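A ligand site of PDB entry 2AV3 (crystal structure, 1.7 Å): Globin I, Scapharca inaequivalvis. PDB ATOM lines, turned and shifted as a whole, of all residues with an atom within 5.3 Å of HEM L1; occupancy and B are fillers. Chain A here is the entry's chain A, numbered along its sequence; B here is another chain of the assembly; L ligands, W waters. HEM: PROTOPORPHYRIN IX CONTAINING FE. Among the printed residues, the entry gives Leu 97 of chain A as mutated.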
ATOM      1  N   LEU A  40      13.384 -28.351  -8.887  1.00  0.00           N
ATOM      2  CA  LEU A  40      13.255 -26.960  -8.469  1.00  0.00           C
ATOM      3  C   LEU A  40      13.892 -26.057  -9.525  1.00  0.00           C
ATOM      4  O   LEU A  40      13.295 -25.063  -9.939  1.00  0.00           O
ATOM      5  CB  LEU A  40      13.940 -26.726  -7.123  1.00  0.00           C
ATOM      6  CG  LEU A  40      13.980 -25.273  -6.650  1.00  0.00           C
ATOM      7  CD1 LEU A  40      12.584 -24.825  -6.209  1.00  0.00           C
ATOM      8  CD2 LEU A  40      14.952 -25.131  -5.496  1.00  0.00           C
ATOM      9  N   THR A  47      15.390 -19.390  -9.323  1.00  0.00           N
ATOM     10  CA  THR A  47      16.015 -19.722  -8.045  1.00  0.00           C
ATOM     11  C   THR A  47      17.473 -20.143  -8.158  1.00  0.00           C
ATOM     12  O   THR A  47      18.178 -20.203  -7.154  1.00  0.00           O
ATOM     13  CB  THR A  47      15.260 -20.848  -7.311  1.00  0.00           C
ATOM     14  OG1 THR A  47      15.338 -22.053  -8.081  1.00  0.00           O
ATOM     15  CG2 THR A  47      13.800 -20.466  -7.092  1.00  0.00           C
ATOM     16  N   TYR A  50      20.511 -18.158  -6.478  1.00  0.00           N
ATOM     17  CA  TYR A  50      20.854 -18.315  -5.063  1.00  0.00           C
ATOM     18  C   TYR A  50      21.868 -19.423  -4.832  1.00  0.00           C
ATOM     19  O   TYR A  50      22.511 -19.474  -3.775  1.00  0.00           O
ATOM     20  CB  TYR A  50      19.595 -18.646  -4.240  1.00  0.00           C
ATOM     21  CG  TYR A  50      18.564 -17.548  -4.176  1.00  0.00           C
ATOM     22  CD1 TYR A  50      18.810 -16.363  -3.478  1.00  0.00           C
ATOM     23  CD2 TYR A  50      17.314 -17.715  -4.780  1.00  0.00           C
ATOM     24  CE1 TYR A  50      17.829 -15.378  -3.375  1.00  0.00           C
ATOM     25  CE2 TYR A  50      16.332 -16.730  -4.677  1.00  0.00           C
ATOM     26  CZ  TYR A  50      16.594 -15.567  -3.972  1.00  0.00           C
ATOM     27  OH  TYR A  50      15.620 -14.611  -3.864  1.00  0.00           O
ATOM     28  N   PHE A  51      22.031 -20.301  -5.817  1.00  0.00           N
ATOM     29  CA  PHE A  51      22.938 -21.445  -5.697  1.00  0.00           C
ATOM     30  C   PHE A  51      24.205 -21.353  -6.539  1.00  0.00           C
ATOM     31  O   PHE A  51      24.715 -22.375  -7.010  1.00  0.00           O
ATOM     32  CB  PHE A  51      22.172 -22.716  -6.054  1.00  0.00           C
ATOM     33  CG  PHE A  51      21.035 -23.027  -5.122  1.00  0.00           C
ATOM     34  CD1 PHE A  51      21.241 -23.750  -3.953  1.00  0.00           C
ATOM     35  CD2 PHE A  51      19.736 -22.596  -5.427  1.00  0.00           C
ATOM     36  CE1 PHE A  51      20.175 -24.055  -3.102  1.00  0.00           C
ATOM     37  CE2 PHE A  51      18.663 -22.890  -4.579  1.00  0.00           C
ATOM     38  CZ  PHE A  51      18.883 -23.630  -3.411  1.00  0.00           C
ATOM     39  N   ARG A  53      27.271 -20.933  -5.738  1.00  0.00           N
ATOM     40  CA  ARG A  53      28.382 -21.720  -5.192  1.00  0.00           C
ATOM     41  C   ARG A  53      28.388 -23.157  -5.687  1.00  0.00           C
ATOM     42  O   ARG A  53      29.451 -23.762  -5.830  1.00  0.00           O
ATOM     43  CB  ARG A  53      28.343 -21.716  -3.666  1.00  0.00           C
ATOM     44  CG  ARG A  53      29.624 -22.253  -3.030  1.00  0.00           C
ATOM     45  CD  ARG A  53      29.472 -22.430  -1.525  1.00  0.00           C
ATOM     46  NE  ARG A  53      28.636 -23.582  -1.187  1.00  0.00           N
ATOM     47  CZ  ARG A  53      29.013 -24.849  -1.321  1.00  0.00           C
ATOM     48  NH1 ARG A  53      30.219 -25.144  -1.786  1.00  0.00           N
ATOM     49  NH2 ARG A  53      28.189 -25.826  -0.958  1.00  0.00           N
ATOM     50  N   LEU A  54      27.200 -23.706  -5.945  1.00  0.00           N
ATOM     51  CA  LEU A  54      27.062 -25.089  -6.405  1.00  0.00           C
ATOM     52  C   LEU A  54      27.603 -25.349  -7.813  1.00  0.00           C
ATOM     53  O   LEU A  54      27.850 -26.494  -8.181  1.00  0.00           O
ATOM     54  CB  LEU A  54      25.599 -25.520  -6.324  1.00  0.00           C
ATOM     55  CG  LEU A  54      25.103 -26.176  -5.032  1.00  0.00           C
ATOM     56  CD1 LEU A  54      25.643 -25.437  -3.820  1.00  0.00           C
ATOM     57  CD2 LEU A  54      23.584 -26.184  -5.034  1.00  0.00           C
ATOM     58  N   HIS A  69      24.710 -30.954  -1.076  1.00  0.00           N
ATOM     59  CA  HIS A  69      23.613 -30.110  -0.621  1.00  0.00           C
ATOM     60  C   HIS A  69      22.300 -30.899  -0.541  1.00  0.00           C
ATOM     61  O   HIS A  69      21.563 -30.806   0.440  1.00  0.00           O
ATOM     62  CB  HIS A  69      23.423 -28.927  -1.565  1.00  0.00           C
ATOM     63  CG  HIS A  69      22.182 -28.136  -1.308  1.00  0.00           C
ATOM     64  ND1 HIS A  69      22.062 -27.327  -0.206  1.00  0.00           N
ATOM     65  CD2 HIS A  69      21.022 -28.112  -2.012  1.00  0.00           C
ATOM     66  CE1 HIS A  69      20.840 -26.827  -0.255  1.00  0.00           C
ATOM     67  NE2 HIS A  69      20.175 -27.275  -1.334  1.00  0.00           N
ATOM     68  N   THR A  72      22.134 -33.377   2.355  1.00  0.00           N
ATOM     69  CA  THR A  72      22.031 -32.606   3.586  1.00  0.00           C
ATOM     70  C   THR A  72      20.625 -32.034   3.783  1.00  0.00           C
ATOM     71  O   THR A  72      20.115 -32.000   4.900  1.00  0.00           O
ATOM     72  CB  THR A  72      23.087 -31.466   3.581  1.00  0.00           C
ATOM     73  OG1 THR A  72      24.400 -32.049   3.502  1.00  0.00           O
ATOM     74  CG2 THR A  72      22.990 -30.612   4.838  1.00  0.00           C
ATOM     75  N   LEU A  73      20.006 -31.597   2.688  1.00  0.00           N
ATOM     76  CA  LEU A  73      18.648 -31.051   2.754  1.00  0.00           C
ATOM     77  C   LEU A  73      17.687 -32.128   3.269  1.00  0.00           C
ATOM     78  O   LEU A  73      16.793 -31.840   4.055  1.00  0.00           O
ATOM     79  CB  LEU A  73      18.191 -30.574   1.368  1.00  0.00           C
ATOM     80  CG  LEU A  73      16.783 -29.988   1.241  1.00  0.00           C
ATOM     81  CD1 LEU A  73      16.766 -28.972   0.113  1.00  0.00           C
ATOM     82  CD2 LEU A  73      15.758 -31.103   0.992  1.00  0.00           C
ATOM     83  N   ALA A  76      17.492 -32.542   6.974  1.00  0.00           N
ATOM     84  CA  ALA A  76      16.766 -31.484   7.674  1.00  0.00           C
ATOM     85  C   ALA A  76      15.304 -31.934   7.719  1.00  0.00           C
ATOM     86  O   ALA A  76      14.605 -31.708   8.705  1.00  0.00           O
ATOM     87  CB  ALA A  76      16.889 -30.147   6.937  1.00  0.00           C
ATOM     88  N   LEU A  77      14.835 -32.571   6.653  1.00  0.00           N
ATOM     89  CA  LEU A  77      13.453 -33.048   6.630  1.00  0.00           C
ATOM     90  C   LEU A  77      13.330 -34.201   7.627  1.00  0.00           C
ATOM     91  O   LEU A  77      12.318 -34.337   8.299  1.00  0.00           O
ATOM     92  CB  LEU A  77      13.053 -33.509   5.233  1.00  0.00           C
ATOM     93  CG  LEU A  77      12.976 -32.372   4.204  1.00  0.00           C
ATOM     94  CD1 LEU A  77      12.534 -32.934   2.858  1.00  0.00           C
ATOM     95  CD2 LEU A  77      11.989 -31.316   4.700  1.00  0.00           C
ATOM     96  N   PHE A  80      12.875 -32.662  10.954  1.00  0.00           N
ATOM     97  CA  PHE A  80      11.497 -32.223  11.147  1.00  0.00           C
ATOM     98  C   PHE A  80      10.534 -33.371  11.463  1.00  0.00           C
ATOM     99  O   PHE A  80       9.745 -33.276  12.396  1.00  0.00           O
ATOM    100  CB  PHE A  80      10.994 -31.452   9.930  1.00  0.00           C
ATOM    101  CG  PHE A  80      11.718 -30.157   9.678  1.00  0.00           C
ATOM    102  CD1 PHE A  80      12.591 -29.629  10.638  1.00  0.00           C
ATOM    103  CD2 PHE A  80      11.530 -29.452   8.494  1.00  0.00           C
ATOM    104  CE1 PHE A  80      13.255 -28.419  10.415  1.00  0.00           C
ATOM    105  CE2 PHE A  80      12.193 -28.237   8.263  1.00  0.00           C
ATOM    106  CZ  PHE A  80      13.052 -27.726   9.226  1.00  0.00           C
ATOM    107  N   LEU A  97      16.744 -23.579  11.364  1.00  0.00           N
ATOM    108  CA  LEU A  97      16.913 -23.698   9.921  1.00  0.00           C
ATOM    109  C   LEU A  97      16.663 -22.355   9.232  1.00  0.00           C
ATOM    110  O   LEU A  97      17.367 -21.983   8.286  1.00  0.00           O
ATOM    111  CB  LEU A  97      15.937 -24.767   9.394  1.00  0.00           C
ATOM    112  CG  LEU A  97      15.936 -25.269   7.945  1.00  0.00           C
ATOM    113  CD1 LEU A  97      15.250 -24.271   7.048  1.00  0.00           C
ATOM    114  CD2 LEU A  97      17.348 -25.568   7.501  1.00  0.00           C
ATOM    115  N   ASN A 100      19.809 -19.177   8.630  1.00  0.00           N
ATOM    116  CA  ASN A 100      20.645 -19.016   7.444  1.00  0.00           C
ATOM    117  C   ASN A 100      19.841 -18.636   6.205  1.00  0.00           C
ATOM    118  O   ASN A 100      20.370 -17.978   5.315  1.00  0.00           O
ATOM    119  CB  ASN A 100      21.447 -20.285   7.159  1.00  0.00           C
ATOM    120  CG  ASN A 100      22.587 -20.477   8.144  1.00  0.00           C
ATOM    121  OD1 ASN A 100      22.911 -19.576   8.924  1.00  0.00           O
ATOM    122  ND2 ASN A 100      23.212 -21.651   8.107  1.00  0.00           N
ATOM    123  N   HIS A 101      18.574 -19.041   6.135  1.00  0.00           N
ATOM    124  CA  HIS A 101      17.771 -18.679   4.980  1.00  0.00           C
ATOM    125  C   HIS A 101      17.404 -17.195   5.045  1.00  0.00           C
ATOM    126  O   HIS A 101      17.304 -16.532   4.022  1.00  0.00           O
ATOM    127  CB  HIS A 101      16.508 -19.560   4.874  1.00  0.00           C
ATOM    128  CG  HIS A 101      16.806 -20.977   4.481  1.00  0.00           C
ATOM    129  ND1 HIS A 101      17.187 -21.961   5.359  1.00  0.00           N
ATOM    130  CD2 HIS A 101      16.831 -21.547   3.248  1.00  0.00           C
ATOM    131  CE1 HIS A 101      17.436 -23.075   4.652  1.00  0.00           C
ATOM    132  NE2 HIS A 101      17.239 -22.886   3.361  1.00  0.00           N
ATOM    133  N   ARG A 104      20.317 -15.250   3.821  1.00  0.00           N
ATOM    134  CA  ARG A 104      20.419 -15.296   2.365  1.00  0.00           C
ATOM    135  C   ARG A 104      19.267 -14.533   1.716  1.00  0.00           C
ATOM    136  O   ARG A 104      19.133 -14.518   0.496  1.00  0.00           O
ATOM    137  CB  ARG A 104      20.411 -16.733   1.872  1.00  0.00           C
ATOM    138  CG  ARG A 104      21.572 -17.551   2.378  1.00  0.00           C
ATOM    139  CD  ARG A 104      21.448 -19.016   1.996  1.00  0.00           C
ATOM    140  NE  ARG A 104      22.512 -19.780   2.636  1.00  0.00           N
ATOM    141  CZ  ARG A 104      22.311 -20.774   3.483  1.00  0.00           C
ATOM    142  NH1 ARG A 104      21.074 -21.154   3.806  1.00  0.00           N
ATOM    143  NH2 ARG A 104      23.352 -21.388   4.031  1.00  0.00           N
ATOM    144  N   ILE A 106      16.035 -15.224   1.766  1.00  0.00           N
ATOM    145  CA  ILE A 106      15.072 -16.109   1.113  1.00  0.00           C
ATOM    146  C   ILE A 106      13.734 -15.830   1.795  1.00  0.00           C
ATOM    147  O   ILE A 106      13.590 -16.050   2.997  1.00  0.00           O
ATOM    148  CB  ILE A 106      15.422 -17.605   1.306  1.00  0.00           C
ATOM    149  CG1 ILE A 106      16.819 -17.905   0.743  1.00  0.00           C
ATOM    150  CG2 ILE A 106      14.382 -18.476   0.616  1.00  0.00           C
ATOM    151  CD1 ILE A 106      16.979 -17.604  -0.721  1.00  0.00           C
ATOM    152  N   GLU A 110       9.520 -17.390  -1.649  1.00  0.00           N
ATOM    153  CA  GLU A 110      10.605 -18.049  -2.367  1.00  0.00           C
ATOM    154  C   GLU A 110      10.761 -19.485  -1.863  1.00  0.00           C
ATOM    155  O   GLU A 110      10.897 -20.425  -2.643  1.00  0.00           O
ATOM    156  CB  GLU A 110      11.919 -17.298  -2.137  1.00  0.00           C
ATOM    157  CG  GLU A 110      12.955 -17.522  -3.207  1.00  0.00           C
ATOM    158  CD  GLU A 110      12.785 -16.562  -4.377  1.00  0.00           C
ATOM    159  OE1 GLU A 110      12.959 -15.339  -4.181  1.00  0.00           O
ATOM    160  OE2 GLU A 110      12.480 -17.039  -5.492  1.00  0.00           O
ATOM    161  N   PHE A 111      10.726 -19.639  -0.543  1.00  0.00           N
ATOM    162  CA  PHE A 111      10.858 -20.946   0.094  1.00  0.00           C
ATOM    163  C   PHE A 111       9.721 -21.859  -0.341  1.00  0.00           C
ATOM    164  O   PHE A 111       9.915 -23.058  -0.567  1.00  0.00           O
ATOM    165  CB  PHE A 111      10.828 -20.786   1.621  1.00  0.00           C
ATOM    166  CG  PHE A 111      11.377 -21.968   2.369  1.00  0.00           C
ATOM    167  CD1 PHE A 111      12.739 -22.072   2.616  1.00  0.00           C
ATOM    168  CD2 PHE A 111      10.530 -22.955   2.836  1.00  0.00           C
ATOM    169  CE1 PHE A 111      13.254 -23.164   3.330  1.00  0.00           C
ATOM    170  CE2 PHE A 111      11.030 -24.058   3.546  1.00  0.00           C
ATOM    171  CZ  PHE A 111      12.399 -24.157   3.796  1.00  0.00           C
ATOM    172  N   ILE A 114       9.359 -24.766  -3.100  1.00  0.00           N
ATOM    173  CA  ILE A 114       9.759 -26.155  -2.956  1.00  0.00           C
ATOM    174  C   ILE A 114       8.546 -27.100  -2.980  1.00  0.00           C
ATOM    175  O   ILE A 114       8.696 -28.304  -3.176  1.00  0.00           O
ATOM    176  CB  ILE A 114      10.557 -26.357  -1.640  1.00  0.00           C
ATOM    177  CG1 ILE A 114      11.353 -27.665  -1.721  1.00  0.00           C
ATOM    178  CG2 ILE A 114       9.622 -26.361  -0.445  1.00  0.00           C
ATOM    179  CD1 ILE A 114      12.471 -27.626  -2.749  1.00  0.00           C
ATOM    180  N   ILE A 118       8.232 -31.070  -4.335  1.00  0.00           N
ATOM    181  CA  ILE A 118       7.813 -32.093  -3.383  1.00  0.00           C
ATOM    182  C   ILE A 118       6.596 -32.841  -3.940  1.00  0.00           C
ATOM    183  O   ILE A 118       6.540 -34.076  -3.891  1.00  0.00           O
ATOM    184  CB  ILE A 118       7.440 -31.482  -2.013  1.00  0.00           C
ATOM    185  CG1 ILE A 118       8.691 -30.906  -1.343  1.00  0.00           C
ATOM    186  CG2 ILE A 118       6.786 -32.546  -1.127  1.00  0.00           C
ATOM    187  CD1 ILE A 118       8.446 -30.306   0.021  1.00  0.00           C
ATOM    188  N   VAL A 139       5.906 -27.292   5.346  1.00  0.00           N
ATOM    189  CA  VAL A 139       6.683 -26.222   4.728  1.00  0.00           C
ATOM    190  C   VAL A 139       6.180 -24.869   5.226  1.00  0.00           C
ATOM    191  O   VAL A 139       6.961 -23.933   5.407  1.00  0.00           O
ATOM    192  CB  VAL A 139       6.602 -26.298   3.179  1.00  0.00           C
ATOM    193  CG1 VAL A 139       7.209 -25.051   2.536  1.00  0.00           C
ATOM    194  CG2 VAL A 139       7.352 -27.539   2.694  1.00  0.00           C
ATOM    195  N   LYS B  96      30.412 -29.882   2.495  1.00  0.00           N
ATOM    196  CA  LYS B  96      29.217 -29.033   2.576  1.00  0.00           C
ATOM    197  C   LYS B  96      29.171 -28.413   3.964  1.00  0.00           C
ATOM    198  O   LYS B  96      29.000 -27.200   4.122  1.00  0.00           O
ATOM    199  CB  LYS B  96      27.967 -29.881   2.345  1.00  0.00           C
ATOM    200  CG  LYS B  96      26.643 -29.227   2.746  1.00  0.00           C
ATOM    201  CD  LYS B  96      26.266 -28.034   1.878  1.00  0.00           C
ATOM    202  CE  LYS B  96      24.858 -27.563   2.216  1.00  0.00           C
ATOM    203  NZ  LYS B  96      24.411 -26.422   1.364  1.00  0.00           N
ATOM    204  N   ASN B 100      30.055 -23.347   5.866  1.00  0.00           N
ATOM    205  CA  ASN B 100      29.631 -22.345   6.834  1.00  0.00           C
ATOM    206  C   ASN B 100      30.592 -22.179   8.004  1.00  0.00           C
ATOM    207  O   ASN B 100      30.680 -21.100   8.592  1.00  0.00           O
ATOM    208  CB  ASN B 100      28.226 -22.660   7.371  1.00  0.00           C
ATOM    209  CG  ASN B 100      27.143 -22.390   6.341  1.00  0.00           C
ATOM    210  OD1 ASN B 100      27.348 -21.669   5.370  1.00  0.00           O
ATOM    211  ND2 ASN B 100      25.967 -22.960   6.569  1.00  0.00           N
HETATM  212  CHA HEM L   1      21.250 -24.424   2.394  1.00  0.00           C
HETATM  213  CHB HEM L   1      17.450 -27.031   3.938  1.00  0.00           C
HETATM  214  CHC HEM L   1      14.639 -24.926   0.600  1.00  0.00           C
HETATM  215  CHD HEM L   1      18.285 -21.905  -0.514  1.00  0.00           C
HETATM  216  C1A HEM L   1      20.455 -25.301   3.136  1.00  0.00           C
HETATM  217  C2A HEM L   1      20.946 -26.241   4.141  1.00  0.00           C
HETATM  218  C3A HEM L   1      19.874 -26.967   4.550  1.00  0.00           C
HETATM  219  C4A HEM L   1      18.725 -26.494   3.815  1.00  0.00           C
HETATM  220  CMA HEM L   1      19.877 -28.075   5.611  1.00  0.00           C
HETATM  221  CAA HEM L   1      22.367 -26.432   4.669  1.00  0.00           C
HETATM  222  CBA HEM L   1      22.632 -25.632   5.946  1.00  0.00           C
HETATM  223  CGA HEM L   1      22.655 -24.131   5.711  1.00  0.00           C
HETATM  224  O1A HEM L   1      23.607 -23.653   5.049  1.00  0.00           O
HETATM  225  O2A HEM L   1      21.723 -23.430   6.165  1.00  0.00           O
HETATM  226  C1B HEM L   1      16.316 -26.678   3.208  1.00  0.00           C
HETATM  227  C2B HEM L   1      15.042 -27.358   3.266  1.00  0.00           C
HETATM  228  C3B HEM L   1      14.254 -26.824   2.264  1.00  0.00           C
HETATM  229  C4B HEM L   1      15.077 -25.790   1.627  1.00  0.00           C
HETATM  230  CMB HEM L   1      14.638 -28.417   4.300  1.00  0.00           C
HETATM  231  CAB HEM L   1      12.911 -27.118   1.943  1.00  0.00           C
HETATM  232  CBB HEM L   1      12.233 -28.377   2.126  1.00  0.00           C
HETATM  233  C1C HEM L   1      15.381 -23.862   0.068  1.00  0.00           C
HETATM  234  C2C HEM L   1      14.897 -22.982  -0.976  1.00  0.00           C
HETATM  235  C3C HEM L   1      15.896 -22.105  -1.277  1.00  0.00           C
HETATM  236  C4C HEM L   1      16.994 -22.454  -0.395  1.00  0.00           C
HETATM  237  CMC HEM L   1      13.526 -23.119  -1.647  1.00  0.00           C
HETATM  238  CAC HEM L   1      15.979 -21.108  -2.256  1.00  0.00           C
HETATM  239  CBC HEM L   1      15.024 -20.832  -3.294  1.00  0.00           C
HETATM  240  C1D HEM L   1      19.410 -22.367   0.138  1.00  0.00           C
HETATM  241  C2D HEM L   1      20.772 -21.954  -0.211  1.00  0.00           C
HETATM  242  C3D HEM L   1      21.595 -22.693   0.561  1.00  0.00           C
HETATM  243  C4D HEM L   1      20.762 -23.546   1.409  1.00  0.00           C
HETATM  244  CMD HEM L   1      21.186 -20.968  -1.305  1.00  0.00           C
HETATM  245  CAD HEM L   1      23.117 -22.665   0.503  1.00  0.00           C
HETATM  246  CBD HEM L   1      23.607 -23.627  -0.571  1.00  0.00           C
HETATM  247  CGD HEM L   1      25.120 -23.737  -0.593  1.00  0.00           C
HETATM  248  O1D HEM L   1      25.794 -22.735  -0.913  1.00  0.00           O
HETATM  249  O2D HEM L   1      25.643 -24.826  -0.297  1.00  0.00           O
HETATM  250  NA  HEM L   1      19.083 -25.427   2.997  1.00  0.00           N
HETATM  251  NB  HEM L   1      16.318 -25.693   2.225  1.00  0.00           N
HETATM  252  NC  HEM L   1      16.666 -23.526   0.426  1.00  0.00           N
HETATM  253  ND  HEM L   1      19.415 -23.346   1.123  1.00  0.00           N
HETATM  254 FE   HEM L   1      17.786 -24.288   1.905  1.00  0.00          FE
HETATM  255  CHA HEM L   2      26.225 -24.418  13.202  1.00  0.00           C
HETATM  256  CHB HEM L   2      27.389 -29.121  12.933  1.00  0.00           C
HETATM  257  CHC HEM L   2      31.197 -28.256  15.848  1.00  0.00           C
HETATM  258  CHD HEM L   2      30.319 -23.501  15.644  1.00  0.00           C
HETATM  259  C1A HEM L   2      26.219 -25.770  12.870  1.00  0.00           C
HETATM  260  C2A HEM L   2      25.177 -26.438  12.092  1.00  0.00           C
HETATM  261  C3A HEM L   2      25.512 -27.755  12.006  1.00  0.00           C
HETATM  262  C4A HEM L   2      26.761 -27.899  12.727  1.00  0.00           C
HETATM  263  CMA HEM L   2      24.786 -28.866  11.240  1.00  0.00           C
HETATM  264  CAA HEM L   2      23.949 -25.802  11.462  1.00  0.00           C
HETATM  265  CBA HEM L   2      24.145 -25.448   9.999  1.00  0.00           C
HETATM  266  CGA HEM L   2      25.146 -24.332   9.811  1.00  0.00           C
HETATM  267  O1A HEM L   2      24.794 -23.166  10.081  1.00  0.00           O
HETATM  268  O2A HEM L   2      26.282 -24.607   9.395  1.00  0.00           O
HETATM  269  C1B HEM L   2      28.574 -29.271  13.662  1.00  0.00           C
HETATM  270  C2B HEM L   2      29.164 -30.572  13.980  1.00  0.00           C
HETATM  271  C3B HEM L   2      30.202 -30.345  14.828  1.00  0.00           C
HETATM  272  C4B HEM L   2      30.256 -28.903  15.029  1.00  0.00           C
HETATM  273  CMB HEM L   2      28.708 -31.899  13.352  1.00  0.00           C
HETATM  274  CAB HEM L   2      31.095 -31.265  15.403  1.00  0.00           C
HETATM  275  CBB HEM L   2      30.823 -32.631  15.767  1.00  0.00           C
HETATM  276  C1C HEM L   2      31.338 -26.882  15.978  1.00  0.00           C
HETATM  277  C2C HEM L   2      32.367 -26.217  16.804  1.00  0.00           C
HETATM  278  C3C HEM L   2      32.158 -24.858  16.714  1.00  0.00           C
HETATM  279  C4C HEM L   2      30.987 -24.718  15.834  1.00  0.00           C
HETATM  280  CMC HEM L   2      33.427 -26.958  17.615  1.00  0.00           C
HETATM  281  CAC HEM L   2      32.839 -23.760  17.278  1.00  0.00           C
HETATM  282  CBC HEM L   2      33.880 -23.744  18.268  1.00  0.00           C
HETATM  283  C1D HEM L   2      29.122 -23.337  14.962  1.00  0.00           C
HETATM  284  C2D HEM L   2      28.375 -22.114  14.969  1.00  0.00           C
HETATM  285  C3D HEM L   2      27.217 -22.364  14.320  1.00  0.00           C
HETATM  286  C4D HEM L   2      27.275 -23.751  13.870  1.00  0.00           C
HETATM  287  CMD HEM L   2      28.797 -20.776  15.599  1.00  0.00           C
HETATM  288  CAD HEM L   2      26.034 -21.415  14.235  1.00  0.00           C
HETATM  289  CBD HEM L   2      25.166 -21.508  15.481  1.00  0.00           C
HETATM  290  CGD HEM L   2      23.926 -20.653  15.396  1.00  0.00           C
HETATM  291  O1D HEM L   2      24.044 -19.417  15.527  1.00  0.00           O
HETATM  292  O2D HEM L   2      22.833 -21.210  15.187  1.00  0.00           O
HETATM  293  NA  HEM L   2      27.222 -26.664  13.189  1.00  0.00           N
HETATM  294  NB  HEM L   2      29.278 -28.256  14.276  1.00  0.00           N
HETATM  295  NC  HEM L   2      30.523 -25.942  15.355  1.00  0.00           N
HETATM  296  ND  HEM L   2      28.444 -24.349  14.297  1.00  0.00           N
HETATM  297 FE   HEM L   2      29.043 -26.268  13.988  1.00  0.00          FE
HETATM  298  O   HOH W   1      17.590 -25.933  -1.202  1.00  0.00           O
HETATM  299  O   HOH W   2      25.849 -24.795   3.267  1.00  0.00           O
HETATM  300  O   HOH W   3      20.105 -23.921   8.148  1.00  0.00           O
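The side-chain amino group (NZ) of Lys 96 of chain B is in salt-bridge range of an oxygen (O2D) of HEM L1 (2.6 Å). The side-chain amide nitrogen (ND2) of Asn 100 of chain B lies within hydrogen-bond range of an oxygen (O1A) of HEM L1, at 2.9 Å. An iron atom (FE) of HEM L1 is bound by a ring nitrogen (NE2) of His 101 (2.1 Å). An oxygen (O2A) of HEM L1 lies within hydrogen-bond range of the side-chain amide nitrogen of Asn 100 of chain A (3.0 Å). O1A of HEM L2 lies within hydrogen-bond range of ND2 of Asn 100 of chain A, at 2.9 Å. O2A of HEM L2 lies within hydrogen-bond range of ND2 of Asn 100 of chain B. The guanidinium group (NH2) of Arg 53 is in salt-bridge range of an oxygen (O2D) of HEM L1 (2.8 Å). An oxygen (O1A) of HEM L1 lies within salt-bridge range of the guanidinium group (NH2) of Arg 104 (2.5 Å).
ND2 of Asn 100 of chain A lies close to ND2 of Asn 100 of chain B (3.4 Å). OE1 of Glu 110 lies within hydrogen-bond range of OH of Tyr 50. The backbone carbonyl oxygen of His 101 is in hydrogen-bond range of the backbone NH of Ile 106, 2.9 Å away. A ring nitrogen (ND1) of His 69 is in hydrogen-bond range of the side-chain amino group (NZ) of Lys 96 of chain B, 3.0 Å away. ND1 of His 101 lies within hydrogen-bond range of O of Leu 97 (2.9 Å).
Merely in contact with HEM L1: Tyr 50 (3.2 Å), Phe 51 (3.4 Å), Leu 54 (3.6 Å), His 69 (3.6 Å), Thr 72 (3.996 Å), Leu 73 (3.7 Å), Ala 76 (3.9 Å), Leu 77 (3.9 Å), Leu 97 (3.9 Å), Ile 106 (3.95 Å), Glu 110 (3.9 Å) and Phe 111 (3.5 Å). Within 4 Å of HEM L1: Tyr 50, Phe 51, Arg 53, Leu 54, His 69, Thr 72, Leu 73, Ala 76, Leu 77, Leu 97, Asn 100 of chain A, His 101, Arg 104, Ile 106, Glu 110, Phe 111, Lys 96 of chain B and Asn 100 of chain B. The nearest printed residue that does not touch HEM L1 is Thr 47 (4.01 Å).
Water W3 bridges O2A of HEM L1 and O of Leu 97. Water W2 lies within hydrogen-bond range of the side-chain amino group (NZ) of Lys 96 of chain B (2.9 Å) and an oxygen (O1A) of HEM L1 (3.1 Å).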
